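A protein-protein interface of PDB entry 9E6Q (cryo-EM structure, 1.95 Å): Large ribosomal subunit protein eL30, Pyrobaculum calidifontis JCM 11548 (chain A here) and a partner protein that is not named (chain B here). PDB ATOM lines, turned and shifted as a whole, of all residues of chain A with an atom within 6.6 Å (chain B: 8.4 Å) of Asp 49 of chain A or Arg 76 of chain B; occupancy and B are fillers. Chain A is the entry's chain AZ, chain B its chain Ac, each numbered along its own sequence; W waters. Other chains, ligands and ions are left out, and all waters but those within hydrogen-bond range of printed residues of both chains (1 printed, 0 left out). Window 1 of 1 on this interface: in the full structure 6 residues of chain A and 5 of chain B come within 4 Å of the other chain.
Hydrophobic or aromatic side chains of chain B that line the printed part of chain A: Tyr 80. Among the printed residues, 10 pairs touch across the chains.
Among the printed residues, merely in contact across the chains: Trp 45 of chain A with Arg 76 of chain B, Trp 45 of chain A with Tyr 80 of chain B, Glu 48 of chain A with Tyr 80 of chain B, Glu 48 of chain A with Arg 83 of chain B and Tyr 52 of chain A with Arg 83 of chain B.
Of the printed residues of chain B, Asp 49 of chain A touches Arg 76 (2.6 Å) and Arg 83 (2.9 Å). Of the printed residues of chain B, Tyr 52 of chain A touches Arg 83. Ser 70 of chain B touches none of the printed residues of chain A. Ala 75 of chain B touches none of the printed residues of chain A. Of the printed residues of chain A, Arg 79 of chain B touches Tyr 53. Printed residues of chain A within 4 Å of Arg 83 of chain B: Glu 48 (3.9 Å), Asp 49 (2.9 Å) and Tyr 52 (3.3 Å). The nearest residue of chain B that does not touch Asp 49 of chain A is Arg 79 of chain B (4.2 Å). The nearest residue of chain A that does not touch Arg 76 of chain B is Lys 25 of chain A (4.4 Å). The nearest printed residue of chain A that does not touch Tyr 80 of chain B is Asp 49 of chain A (4.9 Å).
Water W1 lies within hydrogen-bond range of the guanidinium group of Arg 79 of chain B (2.8 Å) and the side-chain hydroxyl of Tyr 53 of chain A (3.3 Å).
The side-chain hydroxyl (OH) of Tyr 80 of chain B sits at hydrogen-bond distance from the guanidinium group (NH1) of Arg 44 of chain A, at 3.4 Å. OE2 of Glu 48 of chain A lies within salt-bridge range of NH2 of Arg 84 of chain B (3.2 Å). OD2 of Asp 49 of chain A lies within salt-bridge range of NH1 of Arg 76 of chain B. NH2 of Arg 83 of chain B is in salt-bridge range of OD2 of Asp 49 of chain A, at 2.9 Å. NH1 of Arg 79 of chain B lies within hydrogen-bond range of OH of Tyr 53 of chain A (3.3 Å).
NZ of Lys 25 of chain A lies within salt-bridge range of OD1 of Asp 49 of chain A, at 2.8 Å. The guanidinium group (NH1) of Arg 44 of chain A lies within salt-bridge range of the side-chain carboxylate (OE1) of Glu 48 of chain A. O of Tyr 80 of chain B sits at hydrogen-bond distance from NH1 of Arg 84 of chain B (2.9 Å).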
ATOM      1  N   LEU A  21     -16.161   0.728  -4.364  1.00  0.00           N
ATOM      2  CA  LEU A  21     -17.062   1.837  -4.072  1.00  0.00           C
ATOM      3  C   LEU A  21     -17.289   2.717  -5.294  1.00  0.00           C
ATOM      4  O   LEU A  21     -18.422   3.118  -5.574  1.00  0.00           O
ATOM      5  CB  LEU A  21     -16.508   2.671  -2.920  1.00  0.00           C
ATOM      6  CG  LEU A  21     -17.337   3.896  -2.531  1.00  0.00           C
ATOM      7  CD1 LEU A  21     -18.758   3.493  -2.207  1.00  0.00           C
ATOM      8  CD2 LEU A  21     -16.710   4.631  -1.369  1.00  0.00           C
ATOM      9  N   LYS A  25     -20.978   3.118  -7.084  1.00  0.00           N
ATOM     10  CA  LYS A  25     -21.656   4.403  -7.208  1.00  0.00           C
ATOM     11  C   LYS A  25     -22.081   4.660  -8.644  1.00  0.00           C
ATOM     12  O   LYS A  25     -23.189   5.143  -8.895  1.00  0.00           O
ATOM     13  CB  LYS A  25     -20.736   5.520  -6.728  1.00  0.00           C
ATOM     14  CG  LYS A  25     -20.742   5.755  -5.240  1.00  0.00           C
ATOM     15  CD  LYS A  25     -19.656   6.744  -4.864  1.00  0.00           C
ATOM     16  CE  LYS A  25     -20.159   7.784  -3.889  1.00  0.00           C
ATOM     17  NZ  LYS A  25     -19.114   8.792  -3.565  1.00  0.00           N
ATOM     18  N   LEU A  28     -25.125   2.520  -9.502  1.00  0.00           N
ATOM     19  CA  LEU A  28     -26.338   3.082  -8.919  1.00  0.00           C
ATOM     20  C   LEU A  28     -26.807   4.301  -9.701  1.00  0.00           C
ATOM     21  O   LEU A  28     -28.000   4.447  -9.982  1.00  0.00           O
ATOM     22  CB  LEU A  28     -26.097   3.442  -7.454  1.00  0.00           C
ATOM     23  CG  LEU A  28     -26.164   2.283  -6.462  1.00  0.00           C
ATOM     24  CD1 LEU A  28     -25.546   2.675  -5.142  1.00  0.00           C
ATOM     25  CD2 LEU A  28     -27.600   1.846  -6.268  1.00  0.00           C
ATOM     26  N   ARG A  44     -18.209   6.959   7.207  1.00  0.00           N
ATOM     27  CA  ARG A  44     -19.489   7.655   7.256  1.00  0.00           C
ATOM     28  C   ARG A  44     -19.822   8.315   5.927  1.00  0.00           C
ATOM     29  O   ARG A  44     -20.969   8.273   5.473  1.00  0.00           O
ATOM     30  CB  ARG A  44     -19.476   8.696   8.373  1.00  0.00           C
ATOM     31  CG  ARG A  44     -20.835   9.276   8.673  1.00  0.00           C
ATOM     32  CD  ARG A  44     -20.815  10.126   9.936  1.00  0.00           C
ATOM     33  NE  ARG A  44     -20.130  11.408   9.788  1.00  0.00           N
ATOM     34  CZ  ARG A  44     -20.276  12.265   8.783  1.00  0.00           C
ATOM     35  NH1 ARG A  44     -21.179  12.083   7.833  1.00  0.00           N
ATOM     36  NH2 ARG A  44     -19.508  13.349   8.743  1.00  0.00           N
ATOM     37  N   TRP A  45     -18.832   8.941   5.291  1.00  0.00           N
ATOM     38  CA  TRP A  45     -19.087   9.601   4.017  1.00  0.00           C
ATOM     39  C   TRP A  45     -19.506   8.600   2.950  1.00  0.00           C
ATOM     40  O   TRP A  45     -20.398   8.879   2.146  1.00  0.00           O
ATOM     41  CB  TRP A  45     -17.855  10.388   3.570  1.00  0.00           C
ATOM     42  CG  TRP A  45     -16.642   9.551   3.331  1.00  0.00           C
ATOM     43  CD1 TRP A  45     -15.673   9.239   4.231  1.00  0.00           C
ATOM     44  CD2 TRP A  45     -16.263   8.927   2.102  1.00  0.00           C
ATOM     45  NE1 TRP A  45     -14.718   8.454   3.644  1.00  0.00           N
ATOM     46  CE2 TRP A  45     -15.059   8.248   2.335  1.00  0.00           C
ATOM     47  CE3 TRP A  45     -16.832   8.872   0.830  1.00  0.00           C
ATOM     48  CZ2 TRP A  45     -14.413   7.524   1.345  1.00  0.00           C
ATOM     49  CZ3 TRP A  45     -16.188   8.155  -0.149  1.00  0.00           C
ATOM     50  CH2 TRP A  45     -14.992   7.491   0.112  1.00  0.00           C
ATOM     51  N   ALA A  46     -18.875   7.426   2.928  1.00  0.00           N
ATOM     52  CA  ALA A  46     -19.214   6.429   1.920  1.00  0.00           C
ATOM     53  C   ALA A  46     -20.585   5.821   2.176  1.00  0.00           C
ATOM     54  O   ALA A  46     -21.366   5.628   1.241  1.00  0.00           O
ATOM     55  CB  ALA A  46     -18.149   5.341   1.883  1.00  0.00           C
ATOM     56  N   ARG A  47     -20.893   5.515   3.435  1.00  0.00           N
ATOM     57  CA  ARG A  47     -22.187   4.928   3.762  1.00  0.00           C
ATOM     58  C   ARG A  47     -23.327   5.870   3.402  1.00  0.00           C
ATOM     59  O   ARG A  47     -24.334   5.452   2.825  1.00  0.00           O
ATOM     60  CB  ARG A  47     -22.234   4.573   5.244  1.00  0.00           C
ATOM     61  CG  ARG A  47     -23.632   4.371   5.773  1.00  0.00           C
ATOM     62  CD  ARG A  47     -23.656   3.465   6.981  1.00  0.00           C
ATOM     63  NE  ARG A  47     -22.631   3.796   7.964  1.00  0.00           N
ATOM     64  CZ  ARG A  47     -22.575   4.921   8.664  1.00  0.00           C
ATOM     65  NH1 ARG A  47     -23.490   5.868   8.531  1.00  0.00           N
ATOM     66  NH2 ARG A  47     -21.575   5.099   9.520  1.00  0.00           N
ATOM     67  N   GLU A  48     -23.184   7.151   3.736  1.00  0.00           N
ATOM     68  CA  GLU A  48     -24.233   8.116   3.430  1.00  0.00           C
ATOM     69  C   GLU A  48     -24.395   8.297   1.928  1.00  0.00           C
ATOM     70  O   GLU A  48     -25.514   8.457   1.432  1.00  0.00           O
ATOM     71  CB  GLU A  48     -23.927   9.445   4.108  1.00  0.00           C
ATOM     72  CG  GLU A  48     -24.157   9.428   5.599  1.00  0.00           C
ATOM     73  CD  GLU A  48     -23.884  10.765   6.244  1.00  0.00           C
ATOM     74  OE1 GLU A  48     -23.347  10.781   7.370  1.00  0.00           O
ATOM     75  OE2 GLU A  48     -24.195  11.802   5.622  1.00  0.00           O
ATOM     76  N   ASP A  49     -23.289   8.270   1.186  1.00  0.00           N
ATOM     77  CA  ASP A  49     -23.366   8.380  -0.266  1.00  0.00           C
ATOM     78  C   ASP A  49     -24.128   7.208  -0.865  1.00  0.00           C
ATOM     79  O   ASP A  49     -25.028   7.393  -1.689  1.00  0.00           O
ATOM     80  CB  ASP A  49     -21.959   8.457  -0.859  1.00  0.00           C
ATOM     81  CG  ASP A  49     -21.416   9.867  -0.905  1.00  0.00           C
ATOM     82  OD1 ASP A  49     -20.933  10.282  -1.975  1.00  0.00           O
ATOM     83  OD2 ASP A  49     -21.471  10.565   0.125  1.00  0.00           O
ATOM     84  N   ILE A  50     -23.779   5.986  -0.460  1.00  0.00           N
ATOM     85  CA  ILE A  50     -24.460   4.804  -0.978  1.00  0.00           C
ATOM     86  C   ILE A  50     -25.915   4.787  -0.533  1.00  0.00           C
ATOM     87  O   ILE A  50     -26.816   4.482  -1.322  1.00  0.00           O
ATOM     88  CB  ILE A  50     -23.716   3.527  -0.549  1.00  0.00           C
ATOM     89  CG1 ILE A  50     -22.369   3.439  -1.257  1.00  0.00           C
ATOM     90  CG2 ILE A  50     -24.532   2.296  -0.864  1.00  0.00           C
ATOM     91  CD1 ILE A  50     -22.487   3.301  -2.748  1.00  0.00           C
ATOM     92  N   GLU A  51     -26.172   5.126   0.730  1.00  0.00           N
ATOM     93  CA  GLU A  51     -27.544   5.151   1.225  1.00  0.00           C
ATOM     94  C   GLU A  51     -28.395   6.129   0.434  1.00  0.00           C
ATOM     95  O   GLU A  51     -29.544   5.831   0.095  1.00  0.00           O
ATOM     96  CB  GLU A  51     -27.563   5.521   2.705  1.00  0.00           C
ATOM     97  CG  GLU A  51     -27.662   4.344   3.643  1.00  0.00           C
ATOM     98  CD  GLU A  51     -27.201   4.681   5.043  1.00  0.00           C
ATOM     99  OE1 GLU A  51     -27.245   5.870   5.412  1.00  0.00           O
ATOM    100  OE2 GLU A  51     -26.802   3.759   5.782  1.00  0.00           O
ATOM    101  N   TYR A  52     -27.848   7.306   0.138  1.00  0.00           N
ATOM    102  CA  TYR A  52     -28.589   8.314  -0.608  1.00  0.00           C
ATOM    103  C   TYR A  52     -28.833   7.874  -2.045  1.00  0.00           C
ATOM    104  O   TYR A  52     -29.953   7.977  -2.553  1.00  0.00           O
ATOM    105  CB  TYR A  52     -27.824   9.635  -0.574  1.00  0.00           C
ATOM    106  CG  TYR A  52     -28.523  10.778  -1.259  1.00  0.00           C
ATOM    107  CD1 TYR A  52     -29.779  11.196  -0.853  1.00  0.00           C
ATOM    108  CD2 TYR A  52     -27.928  11.433  -2.324  1.00  0.00           C
ATOM    109  CE1 TYR A  52     -30.415  12.236  -1.482  1.00  0.00           C
ATOM    110  CE2 TYR A  52     -28.557  12.472  -2.955  1.00  0.00           C
ATOM    111  CZ  TYR A  52     -29.799  12.870  -2.532  1.00  0.00           C
ATOM    112  OH  TYR A  52     -30.423  13.916  -3.171  1.00  0.00           O
ATOM    113  N   TYR A  53     -27.794   7.387  -2.722  1.00  0.00           N
ATOM    114  CA  TYR A  53     -27.934   7.038  -4.130  1.00  0.00           C
ATOM    115  C   TYR A  53     -28.817   5.814  -4.311  1.00  0.00           C
ATOM    116  O   TYR A  53     -29.633   5.766  -5.235  1.00  0.00           O
ATOM    117  CB  TYR A  53     -26.564   6.796  -4.755  1.00  0.00           C
ATOM    118  CG  TYR A  53     -25.737   8.042  -4.888  1.00  0.00           C
ATOM    119  CD1 TYR A  53     -26.337   9.291  -4.961  1.00  0.00           C
ATOM    120  CD2 TYR A  53     -24.357   7.975  -4.943  1.00  0.00           C
ATOM    121  CE1 TYR A  53     -25.587  10.432  -5.076  1.00  0.00           C
ATOM    122  CE2 TYR A  53     -23.597   9.115  -5.064  1.00  0.00           C
ATOM    123  CZ  TYR A  53     -24.219  10.341  -5.128  1.00  0.00           C
ATOM    124  OH  TYR A  53     -23.469  11.486  -5.248  1.00  0.00           O
ATOM    125  N   ALA A  54     -28.658   4.811  -3.446  1.00  0.00           N
ATOM    126  CA  ALA A  54     -29.482   3.614  -3.547  1.00  0.00           C
ATOM    127  C   ALA A  54     -30.943   3.930  -3.270  1.00  0.00           C
ATOM    128  O   ALA A  54     -31.839   3.318  -3.860  1.00  0.00           O
ATOM    129  CB  ALA A  54     -28.978   2.538  -2.590  1.00  0.00           C
ATOM    130  N   SER B  70      -9.870  23.275  -0.322  1.00  0.00           N
ATOM    131  CA  SER B  70      -9.587  22.561  -1.551  1.00  0.00           C
ATOM    132  C   SER B  70     -10.884  22.159  -2.238  1.00  0.00           C
ATOM    133  O   SER B  70     -11.967  22.206  -1.658  1.00  0.00           O
ATOM    134  CB  SER B  70      -8.733  21.328  -1.266  1.00  0.00           C
ATOM    135  OG  SER B  70      -9.398  20.446  -0.387  1.00  0.00           O
ATOM    136  N   HIS B  71     -10.759  21.773  -3.507  1.00  0.00           N
ATOM    137  CA  HIS B  71     -11.918  21.322  -4.264  1.00  0.00           C
ATOM    138  C   HIS B  71     -12.559  20.104  -3.615  1.00  0.00           C
ATOM    139  O   HIS B  71     -13.782  19.944  -3.656  1.00  0.00           O
ATOM    140  CB  HIS B  71     -11.502  21.005  -5.697  1.00  0.00           C
ATOM    141  CG  HIS B  71     -10.722  19.736  -5.823  1.00  0.00           C
ATOM    142  ND1 HIS B  71      -9.378  19.656  -5.540  1.00  0.00           N
ATOM    143  CD2 HIS B  71     -11.108  18.487  -6.168  1.00  0.00           C
ATOM    144  CE1 HIS B  71      -8.964  18.416  -5.722  1.00  0.00           C
ATOM    145  NE2 HIS B  71      -9.996  17.687  -6.103  1.00  0.00           N
ATOM    146  N   LYS B  72     -11.748  19.231  -3.017  1.00  0.00           N
ATOM    147  CA  LYS B  72     -12.277  18.025  -2.389  1.00  0.00           C
ATOM    148  C   LYS B  72     -13.185  18.361  -1.218  1.00  0.00           C
ATOM    149  O   LYS B  72     -14.239  17.744  -1.041  1.00  0.00           O
ATOM    150  CB  LYS B  72     -11.129  17.133  -1.927  1.00  0.00           C
ATOM    151  CG  LYS B  72     -10.931  15.884  -2.749  1.00  0.00           C
ATOM    152  CD  LYS B  72      -9.854  15.008  -2.142  1.00  0.00           C
ATOM    153  CE  LYS B  72      -8.774  14.683  -3.149  1.00  0.00           C
ATOM    154  NZ  LYS B  72      -7.998  13.477  -2.770  1.00  0.00           N
ATOM    155  N   VAL B  73     -12.780  19.325  -0.393  1.00  0.00           N
ATOM    156  CA  VAL B  73     -13.596  19.730   0.742  1.00  0.00           C
ATOM    157  C   VAL B  73     -14.880  20.394   0.267  1.00  0.00           C
ATOM    158  O   VAL B  73     -15.953  20.166   0.831  1.00  0.00           O
ATOM    159  CB  VAL B  73     -12.786  20.651   1.670  1.00  0.00           C
ATOM    160  CG1 VAL B  73     -13.676  21.268   2.721  1.00  0.00           C
ATOM    161  CG2 VAL B  73     -11.658  19.875   2.316  1.00  0.00           C
ATOM    162  N   LEU B  74     -14.795  21.231  -0.765  1.00  0.00           N
ATOM    163  CA  LEU B  74     -15.980  21.935  -1.240  1.00  0.00           C
ATOM    164  C   LEU B  74     -17.004  20.971  -1.817  1.00  0.00           C
ATOM    165  O   LEU B  74     -18.198  21.073  -1.523  1.00  0.00           O
ATOM    166  CB  LEU B  74     -15.599  22.980  -2.283  1.00  0.00           C
ATOM    167  CG  LEU B  74     -16.831  23.736  -2.778  1.00  0.00           C
ATOM    168  CD1 LEU B  74     -17.418  24.579  -1.665  1.00  0.00           C
ATOM    169  CD2 LEU B  74     -16.532  24.584  -3.991  1.00  0.00           C
ATOM    170  N   ALA B  75     -16.555  20.030  -2.650  1.00  0.00           N
ATOM    171  CA  ALA B  75     -17.481  19.094  -3.277  1.00  0.00           C
ATOM    172  C   ALA B  75     -18.191  18.241  -2.239  1.00  0.00           C
ATOM    173  O   ALA B  75     -19.405  18.040  -2.318  1.00  0.00           O
ATOM    174  CB  ALA B  75     -16.740  18.209  -4.273  1.00  0.00           C
ATOM    175  N   ARG B  76     -17.452  17.738  -1.252  1.00  0.00           N
ATOM    176  CA  ARG B  76     -18.066  16.924  -0.213  1.00  0.00           C
ATOM    177  C   ARG B  76     -19.062  17.735   0.607  1.00  0.00           C
ATOM    178  O   ARG B  76     -20.144  17.246   0.939  1.00  0.00           O
ATOM    179  CB  ARG B  76     -16.982  16.323   0.676  1.00  0.00           C
ATOM    180  CG  ARG B  76     -17.458  15.819   2.017  1.00  0.00           C
ATOM    181  CD  ARG B  76     -18.227  14.519   1.909  1.00  0.00           C
ATOM    182  NE  ARG B  76     -17.930  13.781   0.691  1.00  0.00           N
ATOM    183  CZ  ARG B  76     -18.718  12.850   0.175  1.00  0.00           C
ATOM    184  NH1 ARG B  76     -19.855  12.512   0.754  1.00  0.00           N
ATOM    185  NH2 ARG B  76     -18.356  12.244  -0.951  1.00  0.00           N
ATOM    186  N   ALA B  77     -18.721  18.982   0.928  1.00  0.00           N
ATOM    187  CA  ALA B  77     -19.622  19.810   1.718  1.00  0.00           C
ATOM    188  C   ALA B  77     -20.885  20.155   0.942  1.00  0.00           C
ATOM    189  O   ALA B  77     -21.964  20.276   1.528  1.00  0.00           O
ATOM    190  CB  ALA B  77     -18.906  21.076   2.175  1.00  0.00           C
ATOM    191  N   ILE B  78     -20.772  20.331  -0.374  1.00  0.00           N
ATOM    192  CA  ILE B  78     -21.954  20.588  -1.186  1.00  0.00           C
ATOM    193  C   ILE B  78     -22.827  19.344  -1.270  1.00  0.00           C
ATOM    194  O   ILE B  78     -24.057  19.431  -1.216  1.00  0.00           O
ATOM    195  CB  ILE B  78     -21.542  21.095  -2.579  1.00  0.00           C
ATOM    196  CG1 ILE B  78     -21.003  22.516  -2.481  1.00  0.00           C
ATOM    197  CG2 ILE B  78     -22.710  21.057  -3.531  1.00  0.00           C
ATOM    198  CD1 ILE B  78     -20.533  23.071  -3.794  1.00  0.00           C
ATOM    199  N   ARG B  79     -22.211  18.168  -1.394  1.00  0.00           N
ATOM    200  CA  ARG B  79     -22.984  16.931  -1.412  1.00  0.00           C
ATOM    201  C   ARG B  79     -23.763  16.750  -0.118  1.00  0.00           C
ATOM    202  O   ARG B  79     -24.911  16.298  -0.138  1.00  0.00           O
ATOM    203  CB  ARG B  79     -22.061  15.738  -1.644  1.00  0.00           C
ATOM    204  CG  ARG B  79     -21.659  15.547  -3.079  1.00  0.00           C
ATOM    205  CD  ARG B  79     -20.893  14.264  -3.260  1.00  0.00           C
ATOM    206  NE  ARG B  79     -19.866  14.391  -4.283  1.00  0.00           N
ATOM    207  CZ  ARG B  79     -20.068  14.173  -5.572  1.00  0.00           C
ATOM    208  NH1 ARG B  79     -21.250  13.809  -6.033  1.00  0.00           N
ATOM    209  NH2 ARG B  79     -19.060  14.329  -6.421  1.00  0.00           N
ATOM    210  N   TYR B  80     -23.155  17.092   1.016  1.00  0.00           N
ATOM    211  CA  TYR B  80     -23.860  16.993   2.288  1.00  0.00           C
ATOM    212  C   TYR B  80     -25.043  17.947   2.341  1.00  0.00           C
ATOM    213  O   TYR B  80     -26.103  17.597   2.865  1.00  0.00           O
ATOM    214  CB  TYR B  80     -22.911  17.277   3.446  1.00  0.00           C
ATOM    215  CG  TYR B  80     -22.025  16.122   3.832  1.00  0.00           C
ATOM    216  CD1 TYR B  80     -22.320  14.829   3.437  1.00  0.00           C
ATOM    217  CD2 TYR B  80     -20.893  16.328   4.599  1.00  0.00           C
ATOM    218  CE1 TYR B  80     -21.504  13.773   3.796  1.00  0.00           C
ATOM    219  CE2 TYR B  80     -20.077  15.284   4.960  1.00  0.00           C
ATOM    220  CZ  TYR B  80     -20.388  14.010   4.559  1.00  0.00           C
ATOM    221  OH  TYR B  80     -19.566  12.978   4.924  1.00  0.00           O
ATOM    222  N   ALA B  81     -24.879  19.160   1.813  1.00  0.00           N
ATOM    223  CA  ALA B  81     -25.920  20.171   1.940  1.00  0.00           C
ATOM    224  C   ALA B  81     -27.091  19.894   1.009  1.00  0.00           C
ATOM    225  O   ALA B  81     -28.243  20.170   1.356  1.00  0.00           O
ATOM    226  CB  ALA B  81     -25.337  21.552   1.671  1.00  0.00           C
ATOM    227  N   VAL B  82     -26.817  19.356  -0.178  1.00  0.00           N
ATOM    228  CA  VAL B  82     -27.882  19.041  -1.125  1.00  0.00           C
ATOM    229  C   VAL B  82     -28.852  18.036  -0.520  1.00  0.00           C
ATOM    230  O   VAL B  82     -30.073  18.166  -0.657  1.00  0.00           O
ATOM    231  CB  VAL B  82     -27.274  18.525  -2.441  1.00  0.00           C
ATOM    232  CG1 VAL B  82     -28.283  17.711  -3.224  1.00  0.00           C
ATOM    233  CG2 VAL B  82     -26.764  19.681  -3.265  1.00  0.00           C
ATOM    234  N   ARG B  83     -28.326  17.022   0.160  1.00  0.00           N
ATOM    235  CA  ARG B  83     -29.183  16.038   0.806  1.00  0.00           C
ATOM    236  C   ARG B  83     -29.899  16.617   2.018  1.00  0.00           C
ATOM    237  O   ARG B  83     -31.010  16.191   2.343  1.00  0.00           O
ATOM    238  CB  ARG B  83     -28.352  14.831   1.224  1.00  0.00           C
ATOM    239  CG  ARG B  83     -27.569  14.214   0.094  1.00  0.00           C
ATOM    240  CD  ARG B  83     -26.608  13.169   0.609  1.00  0.00           C
ATOM    241  NE  ARG B  83     -25.636  12.774  -0.401  1.00  0.00           N
ATOM    242  CZ  ARG B  83     -24.442  12.269  -0.137  1.00  0.00           C
ATOM    243  NH1 ARG B  83     -24.026  12.094   1.104  1.00  0.00           N
ATOM    244  NH2 ARG B  83     -23.650  11.923  -1.145  1.00  0.00           N
ATOM    245  N   ARG B  84     -29.285  17.579   2.688  1.00  0.00           N
ATOM    246  CA  ARG B  84     -29.700  17.967   4.022  1.00  0.00           C
ATOM    247  C   ARG B  84     -30.276  19.372   4.058  1.00  0.00           C
ATOM    248  O   ARG B  84     -31.487  19.548   4.161  1.00  0.00           O
ATOM    249  CB  ARG B  84     -28.507  17.860   4.962  1.00  0.00           C
ATOM    250  CG  ARG B  84     -28.832  17.775   6.421  1.00  0.00           C
ATOM    251  CD  ARG B  84     -27.562  17.524   7.221  1.00  0.00           C
ATOM    252  NE  ARG B  84     -27.184  16.115   7.243  1.00  0.00           N
ATOM    253  CZ  ARG B  84     -26.368  15.532   6.374  1.00  0.00           C
ATOM    254  NH1 ARG B  84     -25.833  16.201   5.368  1.00  0.00           N
ATOM    255  NH2 ARG B  84     -26.079  14.242   6.522  1.00  0.00           N
HETATM  256  O   HOH W   1     -21.179  11.582  -7.653  1.00  0.00           O
